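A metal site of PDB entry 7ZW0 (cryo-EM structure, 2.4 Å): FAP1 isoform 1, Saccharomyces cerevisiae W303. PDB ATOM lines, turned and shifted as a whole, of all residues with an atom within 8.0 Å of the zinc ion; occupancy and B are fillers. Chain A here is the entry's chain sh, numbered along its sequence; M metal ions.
The backbone carbonyl oxygen (O) of Val 137 lies within hydrogen-bond range of the backbone NH (N) of Cys 132. The backbone NH of Cys 167 sits at hydrogen-bond distance from the backbone carbonyl oxygen of Gln 152 (3.3 Å). The backbone NH of Gly 151 lies within hydrogen-bond range of the side-chain hydroxyl of Ser 149. SG of Cys 134 sits close to N of Lys 136, at 3.3 Å. The side-chain sulfur (SG) of Cys 167 sits close to the backbone NH (N) of Gly 151 (3.1 Å). OE1 of Gln 152 lies close to O of Cys 150. The side-chain hydroxyl (OG) of Ser 149 sits at hydrogen-bond distance from the side-chain carboxylate (OD2) of Asp 146 (3.0 Å). SG of Cys 167 sits close to OG of Ser 149 (2.8 Å).
OG of Ser 149 touches the zinc ion, 3.997 Å away. Gly 151 touches the zinc ion (N to ZN, 3.7 Å). Gln 152 touches the zinc ion. Within 4 Å of the zinc ion: Cys 132, Cys 134, Ser 149, Cys 150, Gly 151, Gln 152 and Cys 167.
The zinc ion is bound by the side-chain sulfur of Cys 132, the side-chain sulfur of Cys 167, the side-chain sulfur of Cys 150 and the side-chain sulfur of Cys 134.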
ATOM      1  N   THR A 131      12.439 -15.118  32.721  1.00  0.00           N
ATOM      2  CA  THR A 131      12.530 -16.107  31.662  1.00  0.00           C
ATOM      3  C   THR A 131      13.930 -16.592  31.468  1.00  0.00           C
ATOM      4  O   THR A 131      14.869 -16.019  32.009  1.00  0.00           O
ATOM      5  CB  THR A 131      12.029 -15.565  30.316  1.00  0.00           C
ATOM      6  OG1 THR A 131      12.758 -14.374  29.982  1.00  0.00           O
ATOM      7  CG2 THR A 131      10.540 -15.255  30.358  1.00  0.00           C
ATOM      8  N   CYS A 132      14.070 -17.652  30.689  1.00  0.00           N
ATOM      9  CA  CYS A 132      15.401 -18.114  30.375  1.00  0.00           C
ATOM     10  C   CYS A 132      15.961 -17.088  29.438  1.00  0.00           C
ATOM     11  O   CYS A 132      15.210 -16.313  28.840  1.00  0.00           O
ATOM     12  CB  CYS A 132      15.357 -19.468  29.685  1.00  0.00           C
ATOM     13  SG  CYS A 132      16.952 -19.880  28.983  1.00  0.00           S
ATOM     14  N   TRP A 133      17.271 -17.049  29.289  1.00  0.00           N
ATOM     15  CA  TRP A 133      17.856 -16.040  28.456  1.00  0.00           C
ATOM     16  C   TRP A 133      17.292 -16.186  27.063  1.00  0.00           C
ATOM     17  O   TRP A 133      17.035 -15.194  26.397  1.00  0.00           O
ATOM     18  CB  TRP A 133      19.370 -16.147  28.425  1.00  0.00           C
ATOM     19  CG  TRP A 133      20.074 -15.531  29.603  1.00  0.00           C
ATOM     20  CD1 TRP A 133      21.213 -15.987  30.179  1.00  0.00           C
ATOM     21  CD2 TRP A 133      19.704 -14.346  30.323  1.00  0.00           C
ATOM     22  NE1 TRP A 133      21.582 -15.160  31.207  1.00  0.00           N
ATOM     23  CE2 TRP A 133      20.668 -14.157  31.324  1.00  0.00           C
ATOM     24  CE3 TRP A 133      18.653 -13.425  30.219  1.00  0.00           C
ATOM     25  CZ2 TRP A 133      20.623 -13.099  32.221  1.00  0.00           C
ATOM     26  CZ3 TRP A 133      18.602 -12.374  31.112  1.00  0.00           C
ATOM     27  CH2 TRP A 133      19.578 -12.231  32.096  1.00  0.00           C
ATOM     28  N   CYS A 134      17.088 -17.416  26.622  1.00  0.00           N
ATOM     29  CA  CYS A 134      16.471 -17.630  25.321  1.00  0.00           C
ATOM     30  C   CYS A 134      15.059 -17.085  25.273  1.00  0.00           C
ATOM     31  O   CYS A 134      14.653 -16.509  24.263  1.00  0.00           O
ATOM     32  CB  CYS A 134      16.488 -19.103  24.928  1.00  0.00           C
ATOM     33  SG  CYS A 134      15.726 -20.251  26.078  1.00  0.00           S
ATOM     34  N   GLY A 135      14.300 -17.242  26.350  1.00  0.00           N
ATOM     35  CA  GLY A 135      12.917 -16.814  26.336  1.00  0.00           C
ATOM     36  C   GLY A 135      12.102 -17.993  25.907  1.00  0.00           C
ATOM     37  O   GLY A 135      10.892 -18.031  26.129  1.00  0.00           O
ATOM     38  N   LYS A 136      12.753 -18.961  25.277  1.00  0.00           N
ATOM     39  CA  LYS A 136      12.071 -20.174  24.874  1.00  0.00           C
ATOM     40  C   LYS A 136      11.425 -20.790  26.080  1.00  0.00           C
ATOM     41  O   LYS A 136      10.301 -21.299  26.010  1.00  0.00           O
ATOM     42  CB  LYS A 136      13.059 -21.153  24.255  1.00  0.00           C
ATOM     43  CG  LYS A 136      13.810 -20.581  23.060  1.00  0.00           C
ATOM     44  CD  LYS A 136      14.949 -21.486  22.622  1.00  0.00           C
ATOM     45  CE  LYS A 136      14.480 -22.595  21.705  1.00  0.00           C
ATOM     46  NZ  LYS A 136      15.634 -23.299  21.068  1.00  0.00           N
ATOM     47  N   VAL A 137      12.125 -20.756  27.211  1.00  0.00           N
ATOM     48  CA  VAL A 137      11.607 -21.374  28.416  1.00  0.00           C
ATOM     49  C   VAL A 137      11.242 -20.357  29.490  1.00  0.00           C
ATOM     50  O   VAL A 137      12.080 -19.551  29.898  1.00  0.00           O
ATOM     51  CB  VAL A 137      12.640 -22.374  28.998  1.00  0.00           C
ATOM     52  CG1 VAL A 137      12.011 -23.213  30.096  1.00  0.00           C
ATOM     53  CG2 VAL A 137      13.182 -23.266  27.899  1.00  0.00           C
ATOM     54  N   PRO A 140      13.033 -19.906  34.236  1.00  0.00           N
ATOM     55  CA  PRO A 140      14.300 -20.590  34.019  1.00  0.00           C
ATOM     56  C   PRO A 140      14.791 -21.306  35.265  1.00  0.00           C
ATOM     57  O   PRO A 140      14.712 -20.771  36.371  1.00  0.00           O
ATOM     58  CB  PRO A 140      15.254 -19.434  33.715  1.00  0.00           C
ATOM     59  CG  PRO A 140      14.689 -18.278  34.447  1.00  0.00           C
ATOM     60  CD  PRO A 140      13.201 -18.463  34.434  1.00  0.00           C
ATOM     61  N   ASP A 146      24.978 -20.882  34.257  1.00  0.00           N
ATOM     62  CA  ASP A 146      24.379 -19.937  33.327  1.00  0.00           C
ATOM     63  C   ASP A 146      23.236 -19.247  34.059  1.00  0.00           C
ATOM     64  O   ASP A 146      22.144 -19.812  34.162  1.00  0.00           O
ATOM     65  CB  ASP A 146      23.887 -20.664  32.066  1.00  0.00           C
ATOM     66  CG  ASP A 146      23.999 -19.811  30.824  1.00  0.00           C
ATOM     67  OD1 ASP A 146      24.219 -18.583  30.950  1.00  0.00           O
ATOM     68  OD2 ASP A 146      23.844 -20.357  29.708  1.00  0.00           O
ATOM     69  N   PRO A 147      23.462 -18.024  34.530  1.00  0.00           N
ATOM     70  CA  PRO A 147      22.416 -17.364  35.317  1.00  0.00           C
ATOM     71  C   PRO A 147      21.191 -17.075  34.477  1.00  0.00           C
ATOM     72  O   PRO A 147      21.349 -16.651  33.341  1.00  0.00           O
ATOM     73  CB  PRO A 147      23.097 -16.071  35.765  1.00  0.00           C
ATOM     74  CG  PRO A 147      24.551 -16.337  35.670  1.00  0.00           C
ATOM     75  CD  PRO A 147      24.699 -17.226  34.480  1.00  0.00           C
ATOM     76  N   ASN A 148      19.987 -17.283  35.029  1.00  0.00           N
ATOM     77  CA  ASN A 148      18.739 -17.021  34.316  1.00  0.00           C
ATOM     78  C   ASN A 148      18.707 -17.734  32.988  1.00  0.00           C
ATOM     79  O   ASN A 148      18.126 -17.243  32.036  1.00  0.00           O
ATOM     80  CB  ASN A 148      18.544 -15.525  34.065  1.00  0.00           C
ATOM     81  CG  ASN A 148      17.099 -15.095  34.162  1.00  0.00           C
ATOM     82  OD1 ASN A 148      16.388 -15.450  35.108  1.00  0.00           O
ATOM     83  ND2 ASN A 148      16.653 -14.303  33.200  1.00  0.00           N
ATOM     84  N   SER A 149      19.362 -18.881  32.914  1.00  0.00           N
ATOM     85  CA  SER A 149      19.433 -19.554  31.636  1.00  0.00           C
ATOM     86  C   SER A 149      19.275 -21.049  31.639  1.00  0.00           C
ATOM     87  O   SER A 149      19.871 -21.748  32.457  1.00  0.00           O
ATOM     88  CB  SER A 149      20.746 -19.197  30.964  1.00  0.00           C
ATOM     89  OG  SER A 149      20.916 -19.915  29.767  1.00  0.00           O
ATOM     90  N   CYS A 150      18.465 -21.563  30.715  1.00  0.00           N
ATOM     91  CA  CYS A 150      18.347 -23.003  30.561  1.00  0.00           C
ATOM     92  C   CYS A 150      19.703 -23.460  30.074  1.00  0.00           C
ATOM     93  O   CYS A 150      20.171 -24.527  30.445  1.00  0.00           O
ATOM     94  CB  CYS A 150      17.228 -23.378  29.582  1.00  0.00           C
ATOM     95  SG  CYS A 150      17.517 -23.020  27.840  1.00  0.00           S
ATOM     96  N   GLY A 151      20.332 -22.645  29.228  1.00  0.00           N
ATOM     97  CA  GLY A 151      21.631 -22.991  28.683  1.00  0.00           C
ATOM     98  C   GLY A 151      21.551 -23.608  27.311  1.00  0.00           C
ATOM     99  O   GLY A 151      22.572 -23.787  26.654  1.00  0.00           O
ATOM    100  N   GLN A 152      20.350 -23.938  26.852  1.00  0.00           N
ATOM    101  CA  GLN A 152      20.201 -24.451  25.488  1.00  0.00           C
ATOM    102  C   GLN A 152      20.154 -23.306  24.476  1.00  0.00           C
ATOM    103  O   GLN A 152      19.649 -22.238  24.781  1.00  0.00           O
ATOM    104  CB  GLN A 152      18.966 -25.351  25.363  1.00  0.00           C
ATOM    105  CG  GLN A 152      19.186 -26.764  25.868  1.00  0.00           C
ATOM    106  CD  GLN A 152      19.251 -26.843  27.382  1.00  0.00           C
ATOM    107  OE1 GLN A 152      18.413 -26.276  28.086  1.00  0.00           O
ATOM    108  NE2 GLN A 152      20.243 -27.567  27.896  1.00  0.00           N
ATOM    109  N   THR A 153      20.666 -23.540  23.275  1.00  0.00           N
ATOM    110  CA  THR A 153      20.729 -22.481  22.261  1.00  0.00           C
ATOM    111  C   THR A 153      19.486 -21.629  22.099  1.00  0.00           C
ATOM    112  O   THR A 153      18.379 -22.164  21.965  1.00  0.00           O
ATOM    113  CB  THR A 153      21.086 -23.059  20.874  1.00  0.00           C
ATOM    114  OG1 THR A 153      20.136 -24.056  20.505  1.00  0.00           O
ATOM    115  CG2 THR A 153      22.476 -23.672  20.896  1.00  0.00           C
ATOM    116  N   CYS A 154      19.651 -20.319  22.103  1.00  0.00           N
ATOM    117  CA  CYS A 154      18.524 -19.435  21.868  1.00  0.00           C
ATOM    118  C   CYS A 154      17.994 -19.682  20.471  1.00  0.00           C
ATOM    119  O   CYS A 154      16.778 -19.671  20.258  1.00  0.00           O
ATOM    120  CB  CYS A 154      18.923 -17.966  22.049  1.00  0.00           C
ATOM    121  SG  CYS A 154      20.639 -17.603  21.636  1.00  0.00           S
ATOM    122  N   ILE A 166      24.542 -20.470  22.624  1.00  0.00           N
ATOM    123  CA  ILE A 166      23.505 -20.828  23.572  1.00  0.00           C
ATOM    124  C   ILE A 166      22.855 -19.580  24.133  1.00  0.00           C
ATOM    125  O   ILE A 166      23.354 -18.476  23.932  1.00  0.00           O
ATOM    126  CB  ILE A 166      24.079 -21.652  24.737  1.00  0.00           C
ATOM    127  CG1 ILE A 166      25.034 -20.806  25.575  1.00  0.00           C
ATOM    128  CG2 ILE A 166      24.785 -22.886  24.191  1.00  0.00           C
ATOM    129  CD1 ILE A 166      25.575 -21.520  26.784  1.00  0.00           C
ATOM    130  N   CYS A 167      21.731 -19.727  24.818  1.00  0.00           N
ATOM    131  CA  CYS A 167      21.029 -18.545  25.287  1.00  0.00           C
ATOM    132  C   CYS A 167      21.951 -17.718  26.164  1.00  0.00           C
ATOM    133  O   CYS A 167      22.614 -18.251  27.049  1.00  0.00           O
ATOM    134  CB  CYS A 167      19.764 -18.930  26.043  1.00  0.00           C
ATOM    135  SG  CYS A 167      19.865 -20.339  27.164  1.00  0.00           S
ATOM    136  N   HIS A 168      21.978 -16.409  25.936  1.00  0.00           N
ATOM    137  CA  HIS A 168      22.929 -15.557  26.650  1.00  0.00           C
ATOM    138  C   HIS A 168      22.454 -14.152  26.892  1.00  0.00           C
ATOM    139  O   HIS A 168      21.519 -13.689  26.245  1.00  0.00           O
ATOM    140  CB  HIS A 168      24.223 -15.477  25.842  1.00  0.00           C
ATOM    141  CG  HIS A 168      24.010 -15.284  24.372  1.00  0.00           C
ATOM    142  ND1 HIS A 168      23.016 -14.484  23.856  1.00  0.00           N
ATOM    143  CD2 HIS A 168      24.677 -15.785  23.304  1.00  0.00           C
ATOM    144  CE1 HIS A 168      23.066 -14.509  22.538  1.00  0.00           C
ATOM    145  NE2 HIS A 168      24.078 -15.289  22.171  1.00  0.00           N
HETATM  146 ZN    ZN M   1      17.692 -20.747  27.556  1.00  0.00          ZN
